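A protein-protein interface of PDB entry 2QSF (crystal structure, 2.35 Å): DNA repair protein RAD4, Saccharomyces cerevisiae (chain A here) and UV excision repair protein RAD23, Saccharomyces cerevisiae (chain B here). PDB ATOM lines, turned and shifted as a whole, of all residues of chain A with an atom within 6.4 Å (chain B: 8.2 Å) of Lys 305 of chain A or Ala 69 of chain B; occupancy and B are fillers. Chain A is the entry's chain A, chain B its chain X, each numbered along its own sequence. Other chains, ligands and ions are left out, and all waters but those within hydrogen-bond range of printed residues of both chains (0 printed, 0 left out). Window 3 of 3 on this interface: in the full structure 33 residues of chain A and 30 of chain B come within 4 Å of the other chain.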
ATOM      1  N   PHE A 298       6.523  28.010 -27.796  1.00  0.00           N
ATOM      2  CA  PHE A 298       7.036  26.705 -28.184  1.00  0.00           C
ATOM      3  C   PHE A 298       8.553  26.724 -28.357  1.00  0.00           C
ATOM      4  O   PHE A 298       9.225  25.729 -28.083  1.00  0.00           O
ATOM      5  CB  PHE A 298       6.390  26.245 -29.487  1.00  0.00           C
ATOM      6  CG  PHE A 298       6.950  24.959 -30.005  1.00  0.00           C
ATOM      7  CD1 PHE A 298       6.908  23.810 -29.225  1.00  0.00           C
ATOM      8  CD2 PHE A 298       7.535  24.896 -31.262  1.00  0.00           C
ATOM      9  CE1 PHE A 298       7.442  22.614 -29.689  1.00  0.00           C
ATOM     10  CE2 PHE A 298       8.074  23.703 -31.738  1.00  0.00           C
ATOM     11  CZ  PHE A 298       8.026  22.560 -30.950  1.00  0.00           C
ATOM     12  N   GLU A 300      10.559  28.720 -26.727  1.00  0.00           N
ATOM     13  CA  GLU A 300      11.093  28.898 -25.380  1.00  0.00           C
ATOM     14  C   GLU A 300      11.175  27.536 -24.700  1.00  0.00           C
ATOM     15  O   GLU A 300      12.110  27.246 -23.956  1.00  0.00           O
ATOM     16  CB  GLU A 300      10.173  29.826 -24.588  1.00  0.00           C
ATOM     17  CG  GLU A 300      10.390  29.829 -23.084  1.00  0.00           C
ATOM     18  CD  GLU A 300      11.789  30.248 -22.675  1.00  0.00           C
ATOM     19  OE1 GLU A 300      12.385  31.100 -23.367  1.00  0.00           O
ATOM     20  OE2 GLU A 300      12.284  29.738 -21.643  1.00  0.00           O
ATOM     21  N   LYS A 301      10.182  26.699 -24.970  1.00  0.00           N
ATOM     22  CA  LYS A 301      10.114  25.358 -24.406  1.00  0.00           C
ATOM     23  C   LYS A 301      11.132  24.461 -25.115  1.00  0.00           C
ATOM     24  O   LYS A 301      11.953  23.794 -24.477  1.00  0.00           O
ATOM     25  CB  LYS A 301       8.695  24.815 -24.597  1.00  0.00           C
ATOM     26  CG  LYS A 301       8.413  23.480 -23.930  1.00  0.00           C
ATOM     27  CD  LYS A 301       6.953  23.075 -24.122  1.00  0.00           C
ATOM     28  CE  LYS A 301       5.999  24.081 -23.478  1.00  0.00           C
ATOM     29  NZ  LYS A 301       6.143  24.138 -21.991  1.00  0.00           N
ATOM     30  N   TRP A 302      11.065  24.464 -26.442  1.00  0.00           N
ATOM     31  CA  TRP A 302      11.962  23.685 -27.288  1.00  0.00           C
ATOM     32  C   TRP A 302      13.415  23.940 -26.896  1.00  0.00           C
ATOM     33  O   TRP A 302      14.171  23.018 -26.608  1.00  0.00           O
ATOM     34  CB  TRP A 302      11.753  24.096 -28.746  1.00  0.00           C
ATOM     35  CG  TRP A 302      12.526  23.293 -29.746  1.00  0.00           C
ATOM     36  CD1 TRP A 302      12.133  22.128 -30.342  1.00  0.00           C
ATOM     37  CD2 TRP A 302      13.820  23.599 -30.279  1.00  0.00           C
ATOM     38  NE1 TRP A 302      13.100  21.691 -31.218  1.00  0.00           N
ATOM     39  CE2 TRP A 302      14.148  22.576 -31.195  1.00  0.00           C
ATOM     40  CE3 TRP A 302      14.737  24.638 -30.070  1.00  0.00           C
ATOM     41  CZ2 TRP A 302      15.354  22.562 -31.903  1.00  0.00           C
ATOM     42  CZ3 TRP A 302      15.935  24.624 -30.769  1.00  0.00           C
ATOM     43  CH2 TRP A 302      16.231  23.592 -31.675  1.00  0.00           C
ATOM     44  N   PHE A 303      13.794  25.207 -26.877  1.00  0.00           N
ATOM     45  CA  PHE A 303      15.157  25.589 -26.550  1.00  0.00           C
ATOM     46  C   PHE A 303      15.568  25.155 -25.152  1.00  0.00           C
ATOM     47  O   PHE A 303      16.743  24.889 -24.894  1.00  0.00           O
ATOM     48  CB  PHE A 303      15.309  27.110 -26.680  1.00  0.00           C
ATOM     49  CG  PHE A 303      16.718  27.597 -26.527  1.00  0.00           C
ATOM     50  CD1 PHE A 303      17.658  27.357 -27.517  1.00  0.00           C
ATOM     51  CD2 PHE A 303      17.109  28.274 -25.385  1.00  0.00           C
ATOM     52  CE1 PHE A 303      18.969  27.784 -27.371  1.00  0.00           C
ATOM     53  CE2 PHE A 303      18.416  28.706 -25.230  1.00  0.00           C
ATOM     54  CZ  PHE A 303      19.349  28.458 -26.230  1.00  0.00           C
ATOM     55  N   ARG A 304      14.603  25.088 -24.246  1.00  0.00           N
ATOM     56  CA  ARG A 304      14.911  24.708 -22.880  1.00  0.00           C
ATOM     57  C   ARG A 304      15.204  23.219 -22.791  1.00  0.00           C
ATOM     58  O   ARG A 304      15.958  22.784 -21.921  1.00  0.00           O
ATOM     59  CB  ARG A 304      13.768  25.112 -21.949  1.00  0.00           C
ATOM     60  CG  ARG A 304      14.178  25.224 -20.484  1.00  0.00           C
ATOM     61  CD  ARG A 304      15.550  25.901 -20.319  1.00  0.00           C
ATOM     62  NE  ARG A 304      15.627  27.207 -20.975  1.00  0.00           N
ATOM     63  CZ  ARG A 304      16.707  27.991 -20.973  1.00  0.00           C
ATOM     64  NH1 ARG A 304      17.816  27.607 -20.344  1.00  0.00           N
ATOM     65  NH2 ARG A 304      16.681  29.162 -21.605  1.00  0.00           N
ATOM     66  N   LYS A 305      14.628  22.435 -23.698  1.00  0.00           N
ATOM     67  CA  LYS A 305      14.887  20.998 -23.713  1.00  0.00           C
ATOM     68  C   LYS A 305      16.315  20.740 -24.212  1.00  0.00           C
ATOM     69  O   LYS A 305      17.021  19.882 -23.683  1.00  0.00           O
ATOM     70  CB  LYS A 305      13.927  20.276 -24.648  1.00  0.00           C
ATOM     71  CG  LYS A 305      12.455  20.482 -24.364  1.00  0.00           C
ATOM     72  CD  LYS A 305      11.654  19.526 -25.245  1.00  0.00           C
ATOM     73  CE  LYS A 305      10.165  19.788 -25.205  1.00  0.00           C
ATOM     74  NZ  LYS A 305       9.473  18.863 -26.156  1.00  0.00           N
ATOM     75  N   VAL A 306      16.724  21.493 -25.234  1.00  0.00           N
ATOM     76  CA  VAL A 306      18.053  21.358 -25.828  1.00  0.00           C
ATOM     77  C   VAL A 306      19.163  21.693 -24.840  1.00  0.00           C
ATOM     78  O   VAL A 306      20.145  20.963 -24.736  1.00  0.00           O
ATOM     79  CB  VAL A 306      18.211  22.263 -27.088  1.00  0.00           C
ATOM     80  CG1 VAL A 306      19.633  22.171 -27.625  1.00  0.00           C
ATOM     81  CG2 VAL A 306      17.232  21.833 -28.167  1.00  0.00           C
ATOM     82  N   ILE A 307      19.022  22.798 -24.119  1.00  0.00           N
ATOM     83  CA  ILE A 307      20.044  23.162 -23.154  1.00  0.00           C
ATOM     84  C   ILE A 307      20.078  22.138 -22.025  1.00  0.00           C
ATOM     85  O   ILE A 307      21.147  21.814 -21.501  1.00  0.00           O
ATOM     86  CB  ILE A 307      19.804  24.586 -22.592  1.00  0.00           C
ATOM     87  CG1 ILE A 307      20.421  25.608 -23.550  1.00  0.00           C
ATOM     88  CG2 ILE A 307      20.431  24.742 -21.199  1.00  0.00           C
ATOM     89  CD1 ILE A 307      20.338  27.031 -23.070  1.00  0.00           C
ATOM     90  N   THR A 308      18.910  21.614 -21.663  1.00  0.00           N
ATOM     91  CA  THR A 308      18.827  20.621 -20.597  1.00  0.00           C
ATOM     92  C   THR A 308      19.579  19.370 -21.020  1.00  0.00           C
ATOM     93  O   THR A 308      20.408  18.850 -20.277  1.00  0.00           O
ATOM     94  CB  THR A 308      17.356  20.259 -20.282  1.00  0.00           C
ATOM     95  OG1 THR A 308      16.701  21.398 -19.705  1.00  0.00           O
ATOM     96  CG2 THR A 308      17.285  19.092 -19.300  1.00  0.00           C
ATOM     97  N   ALA A 309      19.295  18.909 -22.231  1.00  0.00           N
ATOM     98  CA  ALA A 309      19.940  17.725 -22.773  1.00  0.00           C
ATOM     99  C   ALA A 309      21.457  17.871 -22.876  1.00  0.00           C
ATOM    100  O   ALA A 309      22.158  16.885 -23.092  1.00  0.00           O
ATOM    101  CB  ALA A 309      19.363  17.412 -24.142  1.00  0.00           C
ATOM    102  N   LEU A 310      21.962  19.092 -22.724  1.00  0.00           N
ATOM    103  CA  LEU A 310      23.398  19.349 -22.814  1.00  0.00           C
ATOM    104  C   LEU A 310      23.979  19.781 -21.486  1.00  0.00           C
ATOM    105  O   LEU A 310      25.197  19.894 -21.350  1.00  0.00           O
ATOM    106  CB  LEU A 310      23.695  20.440 -23.856  1.00  0.00           C
ATOM    107  CG  LEU A 310      23.800  20.091 -25.340  1.00  0.00           C
ATOM    108  CD1 LEU A 310      22.650  19.210 -25.732  1.00  0.00           C
ATOM    109  CD2 LEU A 310      23.806  21.374 -26.176  1.00  0.00           C
ATOM    110  N   GLN B  62      10.642  12.813 -42.038  1.00  0.00           N
ATOM    111  CA  GLN B  62      10.152  12.663 -40.665  1.00  0.00           C
ATOM    112  C   GLN B  62      11.039  13.385 -39.659  1.00  0.00           C
ATOM    113  O   GLN B  62      10.625  13.646 -38.527  1.00  0.00           O
ATOM    114  CB  GLN B  62      10.070  11.187 -40.264  1.00  0.00           C
ATOM    115  CG  GLN B  62      10.000  10.213 -41.416  1.00  0.00           C
ATOM    116  CD  GLN B  62      11.324  10.082 -42.142  1.00  0.00           C
ATOM    117  OE1 GLN B  62      12.339   9.709 -41.546  1.00  0.00           O
ATOM    118  NE2 GLN B  62      11.323  10.385 -43.435  1.00  0.00           N
ATOM    119  N   LEU B  63      12.263  13.699 -40.067  1.00  0.00           N
ATOM    120  CA  LEU B  63      13.192  14.380 -39.181  1.00  0.00           C
ATOM    121  C   LEU B  63      12.586  15.682 -38.675  1.00  0.00           C
ATOM    122  O   LEU B  63      12.823  16.091 -37.535  1.00  0.00           O
ATOM    123  CB  LEU B  63      14.502  14.665 -39.911  1.00  0.00           C
ATOM    124  CG  LEU B  63      15.544  15.364 -39.039  1.00  0.00           C
ATOM    125  CD1 LEU B  63      15.898  14.457 -37.874  1.00  0.00           C
ATOM    126  CD2 LEU B  63      16.781  15.706 -39.861  1.00  0.00           C
ATOM    127  N   ARG B  64      11.803  16.326 -39.532  1.00  0.00           N
ATOM    128  CA  ARG B  64      11.144  17.586 -39.202  1.00  0.00           C
ATOM    129  C   ARG B  64      10.385  17.492 -37.884  1.00  0.00           C
ATOM    130  O   ARG B  64      10.651  18.251 -36.953  1.00  0.00           O
ATOM    131  CB  ARG B  64      10.189  17.986 -40.338  1.00  0.00           C
ATOM    132  CG  ARG B  64       9.127  19.021 -39.962  1.00  0.00           C
ATOM    133  CD  ARG B  64       9.405  20.427 -40.493  1.00  0.00           C
ATOM    134  NE  ARG B  64       9.394  20.506 -41.956  1.00  0.00           N
ATOM    135  CZ  ARG B  64       9.057  21.597 -42.647  1.00  0.00           C
ATOM    136  NH1 ARG B  64       8.693  22.703 -42.012  1.00  0.00           N
ATOM    137  NH2 ARG B  64       9.103  21.595 -43.974  1.00  0.00           N
ATOM    138  N   GLU B  65       9.450  16.548 -37.802  1.00  0.00           N
ATOM    139  CA  GLU B  65       8.640  16.366 -36.598  1.00  0.00           C
ATOM    140  C   GLU B  65       9.437  15.977 -35.354  1.00  0.00           C
ATOM    141  O   GLU B  65       9.197  16.502 -34.266  1.00  0.00           O
ATOM    142  CB  GLU B  65       7.552  15.320 -36.845  1.00  0.00           C
ATOM    143  CG  GLU B  65       6.689  15.605 -38.064  1.00  0.00           C
ATOM    144  CD  GLU B  65       7.232  14.959 -39.329  1.00  0.00           C
ATOM    145  OE1 GLU B  65       7.130  13.715 -39.454  1.00  0.00           O
ATOM    146  OE2 GLU B  65       7.764  15.690 -40.194  1.00  0.00           O
ATOM    147  N   HIS B  66      10.390  15.067 -35.506  1.00  0.00           N
ATOM    148  CA  HIS B  66      11.184  14.633 -34.364  1.00  0.00           C
ATOM    149  C   HIS B  66      12.056  15.743 -33.775  1.00  0.00           C
ATOM    150  O   HIS B  66      12.306  15.762 -32.569  1.00  0.00           O
ATOM    151  CB  HIS B  66      12.015  13.409 -34.758  1.00  0.00           C
ATOM    152  CG  HIS B  66      11.179  12.257 -35.231  1.00  0.00           C
ATOM    153  ND1 HIS B  66      11.721  11.087 -35.720  1.00  0.00           N
ATOM    154  CD2 HIS B  66       9.834  12.103 -35.296  1.00  0.00           C
ATOM    155  CE1 HIS B  66      10.747  10.265 -36.069  1.00  0.00           C
ATOM    156  NE2 HIS B  66       9.592  10.856 -35.822  1.00  0.00           N
ATOM    157  N   ILE B  67      12.503  16.675 -34.611  1.00  0.00           N
ATOM    158  CA  ILE B  67      13.321  17.784 -34.133  1.00  0.00           C
ATOM    159  C   ILE B  67      12.456  18.819 -33.422  1.00  0.00           C
ATOM    160  O   ILE B  67      12.868  19.416 -32.433  1.00  0.00           O
ATOM    161  CB  ILE B  67      14.055  18.473 -35.290  1.00  0.00           C
ATOM    162  CG1 ILE B  67      15.058  17.505 -35.906  1.00  0.00           C
ATOM    163  CG2 ILE B  67      14.780  19.718 -34.791  1.00  0.00           C
ATOM    164  CD1 ILE B  67      16.128  17.068 -34.937  1.00  0.00           C
ATOM    165  N   MET B  68      11.252  19.033 -33.938  1.00  0.00           N
ATOM    166  CA  MET B  68      10.328  19.997 -33.353  1.00  0.00           C
ATOM    167  C   MET B  68       9.767  19.466 -32.036  1.00  0.00           C
ATOM    168  O   MET B  68       9.725  20.173 -31.029  1.00  0.00           O
ATOM    169  CB  MET B  68       9.167  20.259 -34.315  1.00  0.00           C
ATOM    170  CG  MET B  68       9.574  20.752 -35.696  1.00  0.00           C
ATOM    171  SD  MET B  68      10.337  22.375 -35.640  1.00  0.00           S
ATOM    172  CE  MET B  68       8.898  23.425 -35.928  1.00  0.00           C
ATOM    173  N   ALA B  69       9.343  18.207 -32.055  1.00  0.00           N
ATOM    174  CA  ALA B  69       8.757  17.568 -30.889  1.00  0.00           C
ATOM    175  C   ALA B  69       9.731  17.116 -29.793  1.00  0.00           C
ATOM    176  O   ALA B  69       9.559  17.480 -28.629  1.00  0.00           O
ATOM    177  CB  ALA B  69       7.905  16.389 -31.346  1.00  0.00           C
ATOM    178  N   ASN B  70      10.746  16.330 -30.157  1.00  0.00           N
ATOM    179  CA  ASN B  70      11.705  15.812 -29.172  1.00  0.00           C
ATOM    180  C   ASN B  70      13.172  16.013 -29.549  1.00  0.00           C
ATOM    181  O   ASN B  70      13.865  15.064 -29.914  1.00  0.00           O
ATOM    182  CB  ASN B  70      11.456  14.318 -28.956  1.00  0.00           C
ATOM    183  CG  ASN B  70       9.992  13.959 -29.074  1.00  0.00           C
ATOM    184  OD1 ASN B  70       9.165  14.425 -28.287  1.00  0.00           O
ATOM    185  ND2 ASN B  70       9.657  13.139 -30.071  1.00  0.00           N
ATOM    186  N   PRO B  71      13.668  17.250 -29.454  1.00  0.00           N
ATOM    187  CA  PRO B  71      15.062  17.527 -29.795  1.00  0.00           C
ATOM    188  C   PRO B  71      16.058  16.841 -28.864  1.00  0.00           C
ATOM    189  O   PRO B  71      17.179  16.546 -29.277  1.00  0.00           O
ATOM    190  CB  PRO B  71      15.135  19.049 -29.707  1.00  0.00           C
ATOM    191  CG  PRO B  71      14.158  19.356 -28.619  1.00  0.00           C
ATOM    192  CD  PRO B  71      12.992  18.473 -28.989  1.00  0.00           C
ATOM    193  N   GLU B  72      15.652  16.592 -27.615  1.00  0.00           N
ATOM    194  CA  GLU B  72      16.523  15.939 -26.628  1.00  0.00           C
ATOM    195  C   GLU B  72      16.840  14.494 -27.002  1.00  0.00           C
ATOM    196  O   GLU B  72      17.831  13.938 -26.545  1.00  0.00           O
ATOM    197  CB  GLU B  72      15.912  15.971 -25.217  1.00  0.00           C
ATOM    198  CG  GLU B  72      14.636  16.788 -25.070  1.00  0.00           C
ATOM    199  CD  GLU B  72      13.394  16.006 -25.449  1.00  0.00           C
ATOM    200  OE1 GLU B  72      13.121  14.979 -24.795  1.00  0.00           O
ATOM    201  OE2 GLU B  72      12.691  16.415 -26.395  1.00  0.00           O
ATOM    202  N   VAL B  73      15.997  13.879 -27.820  1.00  0.00           N
ATOM    203  CA  VAL B  73      16.276  12.514 -28.244  1.00  0.00           C
ATOM    204  C   VAL B  73      17.362  12.568 -29.319  1.00  0.00           C
ATOM    205  O   VAL B  73      18.335  11.821 -29.268  1.00  0.00           O
ATOM    206  CB  VAL B  73      15.031  11.830 -28.823  1.00  0.00           C
ATOM    207  CG1 VAL B  73      15.399  10.455 -29.357  1.00  0.00           C
ATOM    208  CG2 VAL B  73      13.960  11.721 -27.749  1.00  0.00           C
ATOM    209  N   VAL B  75      19.494  14.829 -29.735  1.00  0.00           N
ATOM    210  CA  VAL B  75      20.725  15.227 -29.066  1.00  0.00           C
ATOM    211  C   VAL B  75      21.470  14.055 -28.411  1.00  0.00           C
ATOM    212  O   VAL B  75      22.696  13.955 -28.509  1.00  0.00           O
ATOM    213  CB  VAL B  75      20.442  16.265 -27.983  1.00  0.00           C
ATOM    214  CG1 VAL B  75      21.673  16.426 -27.091  1.00  0.00           C
ATOM    215  CG2 VAL B  75      20.045  17.582 -28.624  1.00  0.00           C
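Phe 298 of chain A touches Met 68 of chain B. CD1 of Trp 302 of chain A touches O of Met 68 of chain B, at 3.2 Å. NE1 of Trp 302 of chain A touches CG of Pro 71 of chain B, 3.7 Å away. Lys 305 of chain A touches Glu 72 of chain B. Val 306 of chain A touches Pro 71 of chain B (CG2 to CB, 3.8 Å). Ala 309 of chain A touches Glu 72 of chain B (CB to CB, 3.9 Å). CB of Ala 309 of chain A touches CG1 of Val 75 of chain B, 3.9 Å away. CD1 of Leu 310 of chain A touches CG1 of Val 75 of chain B, 3.2 Å away.
Hydrophobic or aromatic side chains of chain A that line the printed part of chain B: Phe 298, Trp 302, Val 306, Ala 309 and Leu 310. Along chain A the printed residues that touch a printed residue of chain B span positions 298 to 310. Hydrophobic or aromatic side chains of chain B within 4 Å of the printed part of chain A: Pro 71 and Val 75. Among the printed residues, 10 pairs touch across the chains. Among the printed residues, no Asp or Glu carboxylate lies within 4 Å of a Lys or Arg side-chain nitrogen of the other chain.
Of the printed residues of chain B, Trp 302 of chain A touches Ile 67 (2.6 Å), Met 68 (3.2 Å) and Pro 71 (3.7 Å). Phe 303 of chain A touches none of the printed residues of chain B. Of chain B, only Ala 69 and Glu 72 come within 4 Å of Lys 305 of chain A. Of the printed residues of chain B, Ala 309 of chain A touches Glu 72 and Val 75. His 66 of chain B touches none of the printed residues of chain A. Of chain A, only Lys 305 comes within 4 Å of Ala 69 of chain B. Printed residues of chain A within 4 Å of Glu 72 of chain B: Lys 305 (3.5 Å) and Ala 309 (3.9 Å). Of the printed residues of chain A, Val 75 of chain B touches Ala 309 (3.9 Å) and Leu 310 (3.2 Å). The nearest residue of chain A that does not touch Ala 69 of chain B is Phe 298 of chain A (4.7 Å).
The backbone carbonyl oxygen (O) of Ile 67 of chain B is in hydrogen-bond range of the indole nitrogen (NE1) of Trp 302 of chain A (2.6 Å). NZ of Lys 305 of chain A sits at hydrogen-bond distance from O of Ala 69 of chain B.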
